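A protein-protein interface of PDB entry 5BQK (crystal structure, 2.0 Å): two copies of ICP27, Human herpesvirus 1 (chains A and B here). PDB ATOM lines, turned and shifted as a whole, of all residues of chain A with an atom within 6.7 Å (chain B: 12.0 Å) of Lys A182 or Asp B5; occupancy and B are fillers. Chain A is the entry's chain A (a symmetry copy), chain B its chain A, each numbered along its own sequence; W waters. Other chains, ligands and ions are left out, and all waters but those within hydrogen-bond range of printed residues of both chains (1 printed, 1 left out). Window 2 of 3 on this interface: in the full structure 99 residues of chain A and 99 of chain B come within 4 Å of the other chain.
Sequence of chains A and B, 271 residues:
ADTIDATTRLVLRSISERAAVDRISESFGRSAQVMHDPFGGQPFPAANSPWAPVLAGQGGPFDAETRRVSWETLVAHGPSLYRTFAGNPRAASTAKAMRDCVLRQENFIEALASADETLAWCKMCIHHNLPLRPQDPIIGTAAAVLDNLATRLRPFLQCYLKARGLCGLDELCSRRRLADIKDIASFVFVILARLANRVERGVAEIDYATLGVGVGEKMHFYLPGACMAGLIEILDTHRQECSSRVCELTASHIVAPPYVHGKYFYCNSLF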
ATOM      1  N   ARG A 164      -8.426 -11.499 -23.417  1.00  0.00           N
ATOM      2  CA  ARG A 164      -7.308 -10.556 -23.443  1.00  0.00           C
ATOM      3  C   ARG A 164      -7.369  -9.489 -24.559  1.00  0.00           C
ATOM      4  O   ARG A 164      -6.507  -8.598 -24.588  1.00  0.00           O
ATOM      5  CB  ARG A 164      -5.960 -11.299 -23.643  1.00  0.00           C
ATOM      6  CG  ARG A 164      -5.524 -12.253 -22.543  1.00  0.00           C
ATOM      7  CD  ARG A 164      -4.963 -11.511 -21.361  1.00  0.00           C
ATOM      8  NE  ARG A 164      -6.021 -10.836 -20.639  1.00  0.00           N
ATOM      9  CZ  ARG A 164      -6.950 -11.452 -19.913  1.00  0.00           C
ATOM     10  NH1 ARG A 164      -6.969 -12.783 -19.796  1.00  0.00           N
ATOM     11  NH2 ARG A 164      -7.884 -10.728 -19.289  1.00  0.00           N
ATOM     12  N   LEU A 166      -6.822 -10.372 -27.804  1.00  0.00           N
ATOM     13  CA  LEU A 166      -5.656 -10.573 -28.730  1.00  0.00           C
ATOM     14  C   LEU A 166      -6.072 -11.292 -30.007  1.00  0.00           C
ATOM     15  O   LEU A 166      -7.223 -11.723 -30.108  1.00  0.00           O
ATOM     16  CB  LEU A 166      -4.495 -11.283 -28.027  1.00  0.00           C
ATOM     17  CG  LEU A 166      -3.939 -10.631 -26.756  1.00  0.00           C
ATOM     18  CD1 LEU A 166      -2.953 -11.567 -26.040  1.00  0.00           C
ATOM     19  CD2 LEU A 166      -3.295  -9.230 -27.030  1.00  0.00           C
ATOM     20  N   LEU A 178       6.482  -9.735 -33.274  1.00  0.00           N
ATOM     21  CA  LEU A 178       6.775  -9.431 -31.871  1.00  0.00           C
ATOM     22  C   LEU A 178       5.746  -8.463 -31.249  1.00  0.00           C
ATOM     23  O   LEU A 178       5.316  -8.611 -30.053  1.00  0.00           O
ATOM     24  CB  LEU A 178       8.203  -8.949 -31.709  1.00  0.00           C
ATOM     25  CG  LEU A 178       9.187  -9.942 -32.339  1.00  0.00           C
ATOM     26  CD1 LEU A 178      10.529  -9.183 -32.487  1.00  0.00           C
ATOM     27  CD2 LEU A 178       9.402 -11.305 -31.550  1.00  0.00           C
ATOM     28  N   ALA A 179       5.220  -7.575 -32.107  1.00  0.00           N
ATOM     29  CA  ALA A 179       4.322  -6.486 -31.656  1.00  0.00           C
ATOM     30  C   ALA A 179       2.976  -7.054 -31.275  1.00  0.00           C
ATOM     31  O   ALA A 179       2.219  -6.396 -30.593  1.00  0.00           O
ATOM     32  CB  ALA A 179       4.252  -5.298 -32.693  1.00  0.00           C
ATOM     33  N   ASP A 180       2.731  -8.347 -31.594  1.00  0.00           N
ATOM     34  CA  ASP A 180       1.501  -9.035 -31.144  1.00  0.00           C
ATOM     35  C   ASP A 180       1.617  -9.612 -29.726  1.00  0.00           C
ATOM     36  O   ASP A 180       0.610 -10.029 -29.123  1.00  0.00           O
ATOM     37  CB  ASP A 180       1.123 -10.172 -32.093  1.00  0.00           C
ATOM     38  CG  ASP A 180       0.567  -9.677 -33.452  1.00  0.00           C
ATOM     39  OD1 ASP A 180       0.291  -8.476 -33.562  1.00  0.00           O
ATOM     40  OD2 ASP A 180       0.375 -10.504 -34.390  1.00  0.00           O
ATOM     41  N   ILE A 181       2.836  -9.747 -29.236  1.00  0.00           N
ATOM     42  CA  ILE A 181       3.071 -10.337 -27.907  1.00  0.00           C
ATOM     43  C   ILE A 181       2.626  -9.311 -26.855  1.00  0.00           C
ATOM     44  O   ILE A 181       3.187  -8.201 -26.834  1.00  0.00           O
ATOM     45  CB  ILE A 181       4.562 -10.779 -27.740  1.00  0.00           C
ATOM     46  CG1 ILE A 181       4.865 -11.852 -28.812  1.00  0.00           C
ATOM     47  CG2 ILE A 181       4.812 -11.296 -26.315  1.00  0.00           C
ATOM     48  CD1 ILE A 181       6.301 -12.143 -28.972  1.00  0.00           C
ATOM     49  N   LYS A 182       1.607  -9.688 -26.069  1.00  0.00           N
ATOM     50  CA  LYS A 182       0.982  -8.857 -25.013  1.00  0.00           C
ATOM     51  C   LYS A 182       0.845  -9.591 -23.669  1.00  0.00           C
ATOM     52  O   LYS A 182       0.463  -8.990 -22.630  1.00  0.00           O
ATOM     53  CB  LYS A 182      -0.409  -8.313 -25.446  1.00  0.00           C
ATOM     54  CG  LYS A 182      -0.436  -7.200 -26.506  1.00  0.00           C
ATOM     55  CD  LYS A 182       0.570  -6.071 -26.266  1.00  0.00           C
ATOM     56  CE  LYS A 182       0.407  -4.946 -27.312  1.00  0.00           C
ATOM     57  NZ  LYS A 182       1.780  -4.444 -27.762  1.00  0.00           N
ATOM     58  N   ASP A 183       1.185 -10.892 -23.657  1.00  0.00           N
ATOM     59  CA  ASP A 183       1.091 -11.722 -22.449  1.00  0.00           C
ATOM     60  C   ASP A 183       1.966 -13.005 -22.604  1.00  0.00           C
ATOM     61  O   ASP A 183       2.754 -13.135 -23.545  1.00  0.00           O
ATOM     62  CB  ASP A 183      -0.403 -12.100 -22.199  1.00  0.00           C
ATOM     63  CG  ASP A 183      -0.841 -13.339 -23.004  1.00  0.00           C
ATOM     64  OD1 ASP A 183      -0.627 -13.389 -24.243  1.00  0.00           O
ATOM     65  OD2 ASP A 183      -1.437 -14.277 -22.416  1.00  0.00           O
ATOM     66  N   ILE A 184       1.814 -13.940 -21.682  1.00  0.00           N
ATOM     67  CA  ILE A 184       2.677 -15.124 -21.672  1.00  0.00           C
ATOM     68  C   ILE A 184       2.282 -16.115 -22.782  1.00  0.00           C
ATOM     69  O   ILE A 184       3.131 -16.674 -23.428  1.00  0.00           O
ATOM     70  CB  ILE A 184       2.704 -15.792 -20.279  1.00  0.00           C
ATOM     71  CG1 ILE A 184       3.703 -17.002 -20.248  1.00  0.00           C
ATOM     72  CG2 ILE A 184       1.280 -16.210 -19.947  1.00  0.00           C
ATOM     73  CD1 ILE A 184       5.120 -16.612 -20.575  1.00  0.00           C
ATOM     74  N   SER A 186       0.600 -15.403 -25.741  1.00  0.00           N
ATOM     75  CA  SER A 186       1.070 -14.882 -27.019  1.00  0.00           C
ATOM     76  C   SER A 186       2.570 -14.978 -27.107  1.00  0.00           C
ATOM     77  O   SER A 186       3.111 -15.282 -28.175  1.00  0.00           O
ATOM     78  CB  SER A 186       0.596 -13.412 -27.270  1.00  0.00           C
ATOM     79  OG  SER A 186       0.949 -12.588 -26.163  1.00  0.00           O
ATOM     80  N   PHE A 187       3.277 -14.730 -26.008  1.00  0.00           N
ATOM     81  CA  PHE A 187       4.747 -14.825 -26.031  1.00  0.00           C
ATOM     82  C   PHE A 187       5.184 -16.246 -26.443  1.00  0.00           C
ATOM     83  O   PHE A 187       5.955 -16.422 -27.342  1.00  0.00           O
ATOM     84  CB  PHE A 187       5.343 -14.488 -24.655  1.00  0.00           C
ATOM     85  CG  PHE A 187       6.877 -14.739 -24.563  1.00  0.00           C
ATOM     86  CD1 PHE A 187       7.784 -13.814 -25.101  1.00  0.00           C
ATOM     87  CD2 PHE A 187       7.383 -15.900 -23.992  1.00  0.00           C
ATOM     88  CE1 PHE A 187       9.182 -14.024 -25.040  1.00  0.00           C
ATOM     89  CE2 PHE A 187       8.792 -16.140 -23.931  1.00  0.00           C
ATOM     90  CZ  PHE A 187       9.695 -15.165 -24.453  1.00  0.00           C
ATOM     91  N   ALA B   1       9.731  -0.637 -36.367  1.00  0.00           N
ATOM     92  CA  ALA B   1      10.557  -1.855 -36.117  1.00  0.00           C
ATOM     93  C   ALA B   1       9.794  -2.817 -35.163  1.00  0.00           C
ATOM     94  O   ALA B   1       9.321  -2.411 -34.080  1.00  0.00           O
ATOM     95  CB  ALA B   1      11.939  -1.459 -35.547  1.00  0.00           C
ATOM     96  N   ASP B   2       9.619  -4.062 -35.596  1.00  0.00           N
ATOM     97  CA  ASP B   2       8.836  -5.064 -34.850  1.00  0.00           C
ATOM     98  C   ASP B   2       9.589  -5.364 -33.548  1.00  0.00           C
ATOM     99  O   ASP B   2      10.769  -5.687 -33.559  1.00  0.00           O
ATOM    100  CB  ASP B   2       8.691  -6.332 -35.705  1.00  0.00           C
ATOM    101  CG  ASP B   2       7.692  -7.355 -35.120  1.00  0.00           C
ATOM    102  OD1 ASP B   2       6.630  -6.988 -34.560  1.00  0.00           O
ATOM    103  OD2 ASP B   2       7.959  -8.554 -35.288  1.00  0.00           O
ATOM    104  N   THR B   3       8.919  -5.227 -32.414  1.00  0.00           N
ATOM    105  CA  THR B   3       9.601  -5.392 -31.152  1.00  0.00           C
ATOM    106  C   THR B   3       8.552  -5.811 -30.103  1.00  0.00           C
ATOM    107  O   THR B   3       7.341  -5.552 -30.246  1.00  0.00           O
ATOM    108  CB  THR B   3      10.344  -4.094 -30.699  1.00  0.00           C
ATOM    109  OG1 THR B   3      11.332  -4.429 -29.695  1.00  0.00           O
ATOM    110  CG2 THR B   3       9.358  -3.086 -30.137  1.00  0.00           C
ATOM    111  N   ILE B   4       9.009  -6.511 -29.083  1.00  0.00           N
ATOM    112  CA  ILE B   4       8.205  -6.713 -27.916  1.00  0.00           C
ATOM    113  C   ILE B   4       8.156  -5.388 -27.077  1.00  0.00           C
ATOM    114  O   ILE B   4       9.184  -4.958 -26.528  1.00  0.00           O
ATOM    115  CB  ILE B   4       8.815  -7.809 -27.025  1.00  0.00           C
ATOM    116  CG1 ILE B   4       8.842  -9.170 -27.746  1.00  0.00           C
ATOM    117  CG2 ILE B   4       7.945  -7.908 -25.773  1.00  0.00           C
ATOM    118  CD1 ILE B   4       9.652 -10.261 -26.920  1.00  0.00           C
ATOM    119  N   ASP B   5       6.977  -4.822 -26.877  1.00  0.00           N
ATOM    120  CA  ASP B   5       6.890  -3.458 -26.263  1.00  0.00           C
ATOM    121  C   ASP B   5       7.330  -3.493 -24.808  1.00  0.00           C
ATOM    122  O   ASP B   5       7.313  -4.584 -24.167  1.00  0.00           O
ATOM    123  CB  ASP B   5       5.471  -2.855 -26.384  1.00  0.00           C
ATOM    124  CG  ASP B   5       4.454  -3.603 -25.495  1.00  0.00           C
ATOM    125  OD1 ASP B   5       4.261  -3.196 -24.294  1.00  0.00           O
ATOM    126  OD2 ASP B   5       3.853  -4.616 -25.995  1.00  0.00           O
ATOM    127  N   ALA B   6       7.758  -2.325 -24.298  1.00  0.00           N
ATOM    128  CA  ALA B   6       8.289  -2.155 -22.945  1.00  0.00           C
ATOM    129  C   ALA B   6       7.379  -2.707 -21.840  1.00  0.00           C
ATOM    130  O   ALA B   6       7.831  -3.332 -20.863  1.00  0.00           O
ATOM    131  CB  ALA B   6       8.562  -0.619 -22.677  1.00  0.00           C
ATOM    132  N   THR B   7       6.092  -2.482 -21.994  1.00  0.00           N
ATOM    133  CA  THR B   7       5.150  -2.841 -20.944  1.00  0.00           C
ATOM    134  C   THR B   7       5.014  -4.385 -20.855  1.00  0.00           C
ATOM    135  O   THR B   7       4.890  -4.966 -19.778  1.00  0.00           O
ATOM    136  CB  THR B   7       3.783  -2.123 -21.201  1.00  0.00           C
ATOM    137  OG1 THR B   7       3.943  -0.734 -20.910  1.00  0.00           O
ATOM    138  CG2 THR B   7       2.694  -2.661 -20.300  1.00  0.00           C
ATOM    139  N   THR B   8       5.045  -5.025 -22.023  1.00  0.00           N
ATOM    140  CA  THR B   8       4.862  -6.468 -22.113  1.00  0.00           C
ATOM    141  C   THR B   8       6.091  -7.146 -21.518  1.00  0.00           C
ATOM    142  O   THR B   8       5.959  -8.136 -20.801  1.00  0.00           O
ATOM    143  CB  THR B   8       4.612  -6.886 -23.553  1.00  0.00           C
ATOM    144  OG1 THR B   8       3.328  -6.387 -23.946  1.00  0.00           O
ATOM    145  CG2 THR B   8       4.669  -8.477 -23.711  1.00  0.00           C
ATOM    146  N   ARG B   9       7.268  -6.580 -21.756  1.00  0.00           N
ATOM    147  CA  ARG B   9       8.456  -7.065 -21.079  1.00  0.00           C
ATOM    148  C   ARG B   9       8.300  -7.073 -19.562  1.00  0.00           C
ATOM    149  O   ARG B   9       8.783  -8.000 -18.910  1.00  0.00           O
ATOM    150  CB  ARG B   9       9.684  -6.247 -21.473  1.00  0.00           C
ATOM    151  CG  ARG B   9      10.070  -6.501 -22.940  1.00  0.00           C
ATOM    152  CD  ARG B   9      11.150  -5.564 -23.368  1.00  0.00           C
ATOM    153  NE  ARG B   9      11.202  -5.381 -24.803  1.00  0.00           N
ATOM    154  CZ  ARG B   9      12.316  -5.528 -25.501  1.00  0.00           C
ATOM    155  NH1 ARG B   9      13.423  -5.899 -24.866  1.00  0.00           N
ATOM    156  NH2 ARG B   9      12.341  -5.285 -26.810  1.00  0.00           N
ATOM    157  N   LEU B  10       7.645  -6.050 -18.995  1.00  0.00           N
ATOM    158  CA  LEU B  10       7.416  -6.014 -17.542  1.00  0.00           C
ATOM    159  C   LEU B  10       6.429  -7.099 -17.175  1.00  0.00           C
ATOM    160  O   LEU B  10       6.630  -7.807 -16.204  1.00  0.00           O
ATOM    161  CB  LEU B  10       6.847  -4.658 -17.046  1.00  0.00           C
ATOM    162  CG  LEU B  10       7.678  -3.394 -17.303  1.00  0.00           C
ATOM    163  CD1 LEU B  10       6.812  -2.121 -16.959  1.00  0.00           C
ATOM    164  CD2 LEU B  10       8.997  -3.468 -16.502  1.00  0.00           C
ATOM    165  N   VAL B  11       5.342  -7.161 -17.926  1.00  0.00           N
ATOM    166  CA  VAL B  11       4.378  -8.225 -17.749  1.00  0.00           C
ATOM    167  C   VAL B  11       5.064  -9.610 -17.719  1.00  0.00           C
ATOM    168  O   VAL B  11       4.817 -10.388 -16.817  1.00  0.00           O
ATOM    169  CB  VAL B  11       3.299  -8.197 -18.828  1.00  0.00           C
ATOM    170  CG1 VAL B  11       2.349  -9.435 -18.691  1.00  0.00           C
ATOM    171  CG2 VAL B  11       2.491  -6.897 -18.735  1.00  0.00           C
ATOM    172  N   LEU B  12       5.938  -9.882 -18.700  1.00  0.00           N
ATOM    173  CA  LEU B  12       6.682 -11.170 -18.774  1.00  0.00           C
ATOM    174  C   LEU B  12       7.576 -11.435 -17.566  1.00  0.00           C
ATOM    175  O   LEU B  12       7.523 -12.527 -16.974  1.00  0.00           O
ATOM    176  CB  LEU B  12       7.485 -11.251 -20.079  1.00  0.00           C
ATOM    177  CG  LEU B  12       6.648 -11.198 -21.353  1.00  0.00           C
ATOM    178  CD1 LEU B  12       7.567 -11.381 -22.578  1.00  0.00           C
ATOM    179  CD2 LEU B  12       5.617 -12.356 -21.312  1.00  0.00           C
ATOM    180  N   ARG B  13       8.386 -10.442 -17.174  1.00  0.00           N
ATOM    181  CA  ARG B  13       9.192 -10.633 -15.982  1.00  0.00           C
ATOM    182  C   ARG B  13       8.372 -10.777 -14.678  1.00  0.00           C
ATOM    183  O   ARG B  13       8.823 -11.413 -13.728  1.00  0.00           O
ATOM    184  CB  ARG B  13      10.287  -9.579 -15.839  1.00  0.00           C
ATOM    185  CG  ARG B  13      11.155  -9.424 -17.110  1.00  0.00           C
ATOM    186  CD  ARG B  13      11.865  -8.047 -17.149  1.00  0.00           C
ATOM    187  NE  ARG B  13      12.303  -7.752 -15.795  1.00  0.00           N
ATOM    188  CZ  ARG B  13      12.002  -6.640 -15.095  1.00  0.00           C
ATOM    189  NH1 ARG B  13      12.437  -6.536 -13.847  1.00  0.00           N
ATOM    190  NH2 ARG B  13      11.309  -5.615 -15.632  1.00  0.00           N
ATOM    191  N   SER B  14       7.148 -10.260 -14.647  1.00  0.00           N
ATOM    192  CA  SER B  14       6.449 -10.194 -13.337  1.00  0.00           C
ATOM    193  C   SER B  14       5.924 -11.583 -12.890  1.00  0.00           C
ATOM    194  O   SER B  14       5.409 -11.735 -11.791  1.00  0.00           O
ATOM    195  CB  SER B  14       5.299  -9.183 -13.402  1.00  0.00           C
ATOM    196  OG  SER B  14       4.165  -9.788 -14.057  1.00  0.00           O
ATOM    197  N   ILE B  15       6.033 -12.601 -13.750  1.00  0.00           N
ATOM    198  CA  ILE B  15       5.645 -13.962 -13.362  1.00  0.00           C
ATOM    199  C   ILE B  15       6.542 -14.365 -12.151  1.00  0.00           C
ATOM    200  O   ILE B  15       6.109 -15.032 -11.210  1.00  0.00           O
ATOM    201  CB  ILE B  15       5.884 -14.894 -14.553  1.00  0.00           C
ATOM    202  CG1 ILE B  15       5.544 -16.348 -14.219  1.00  0.00           C
ATOM    203  CG2 ILE B  15       7.374 -14.835 -14.915  1.00  0.00           C
ATOM    204  CD1 ILE B  15       4.036 -16.540 -13.858  1.00  0.00           C
ATOM    205  N   ARG B  18       5.142 -13.710  -8.816  1.00  0.00           N
ATOM    206  CA  ARG B  18       4.049 -14.563  -8.285  1.00  0.00           C
ATOM    207  C   ARG B  18       4.291 -16.086  -8.244  1.00  0.00           C
ATOM    208  O   ARG B  18       3.590 -16.800  -7.507  1.00  0.00           O
ATOM    209  CB  ARG B  18       2.692 -14.230  -8.956  1.00  0.00           C
ATOM    210  CG  ARG B  18       2.377 -12.679  -9.166  1.00  0.00           C
ATOM    211  CD  ARG B  18       1.107 -12.441 -10.082  1.00  0.00           C
ATOM    212  NE  ARG B  18       1.246 -13.021 -11.424  1.00  0.00           N
ATOM    213  CZ  ARG B  18       1.860 -12.449 -12.478  1.00  0.00           C
ATOM    214  NH1 ARG B  18       1.943 -13.107 -13.643  1.00  0.00           N
ATOM    215  NH2 ARG B  18       2.415 -11.243 -12.399  1.00  0.00           N
HETATM  216  O   HOH W   1       1.059  -6.345 -22.302  1.00  0.00           O
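Water W1 bridges O of Lys A182 (2.7 Å) and OG1 of Thr B8 (2.8 Å).
The backbone NH (N) of Leu A178 is in hydrogen-bond range of the side-chain carboxylate (OD2) of Asp B2 (2.8 Å).
OD2 of Asp B5 lies within salt-bridge range of NZ of Lys A182.
The side-chain carboxylate of Asp B2 is in hydrogen-bond range of the backbone NH of Ala A179 (2.9 Å).
The backbone carbonyl oxygen of Thr B3 sits close to the backbone NH of Ala A179.
The backbone carbonyl oxygen of Ile A181 is in hydrogen-bond range of the side-chain hydroxyl of Thr B8 (3.4 Å).
No position is printed for both chains.
Of the 11 pairs that touch across the chains among the printed residues, none has its exchanged pair printed and touching as well.
Leu A166 touches none of the printed residues of chain B.
Printed residues of chain B within 4 Å of Ala A179: Asp B2 (2.9 Å) and Thr B3 (3.5 Å).
Lys A182 touches two residues of chain B.
Asp A183 touches one residue of chain B.
No residue of chain B comes within 4 Å of Ser A186.
Of the printed residues of chain A, Ile B4 touches Leu A178 (3.7 Å).
Asp B5 touches just these residues of chain A: Ile A181 (3.7 Å) and Lys A182 (2.7 Å).
Printed residues of chain A within 4 Å of Thr B8: Ile A181 and Lys A182.
Of the printed residues of chain A, Leu B12 touches Asp A183 and Phe A187.
Thr B3 touches Leu A178.
Leu A178 touches Ile B4.
O of Ile A181 touches OD2 of Asp B5 (3.7 Å).
Thr B8 touches Lys A182.
Leu B12 touches Asp A183.
Phe A187 touches Leu B12 (CD1 to CD1, 3.5 Å).
The side-chain hydroxyl of Thr B8 sits at hydrogen-bond distance from the side-chain carboxylate of Asp B5 (2.8 Å).
The side-chain hydroxyl of Ser A186 lies within hydrogen-bond range of the backbone NH of Lys A182, 3.0 Å away.
The side-chain carboxylate (OD1) of Asp B5 is in hydrogen-bond range of the backbone NH (N) of Thr B7 (3.0 Å).
The side-chain hydroxyl of Thr B3 lies within hydrogen-bond range of the guanidinium group of Arg B9 (3.2 Å).
O of Ile B4 lies within hydrogen-bond range of NE of Arg B9, 2.7 Å away.
O of Ala A179 lies within hydrogen-bond range of NZ of Lys A182 (3.5 Å).
Of the 16 printed residues of chain B, 6 touch a printed residue of chain A.
Printed residues of chain B that touch a printed residue of chain A: Asp B2, Thr B3, Ile B4, Asp B5, Thr B8 and Leu B12.
Of the 11 printed residues of chain A, 6 touch a printed residue of chain B.
Printed residues of chain A that touch a printed residue of chain B: Leu A178, Ala A179, Ile A181, Lys A182, Asp A183 and Phe A187.
Hydrophobic or aromatic side chains of chain A that line the printed part of chain B: Leu A178, Ala A179, Ile A181 and Phe A187.
Among the printed residues, Asp or Glu carboxylates within 4 Å of a Lys or Arg side-chain nitrogen of the other chain: Lys A182 with Asp B5 (2.7 Å).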
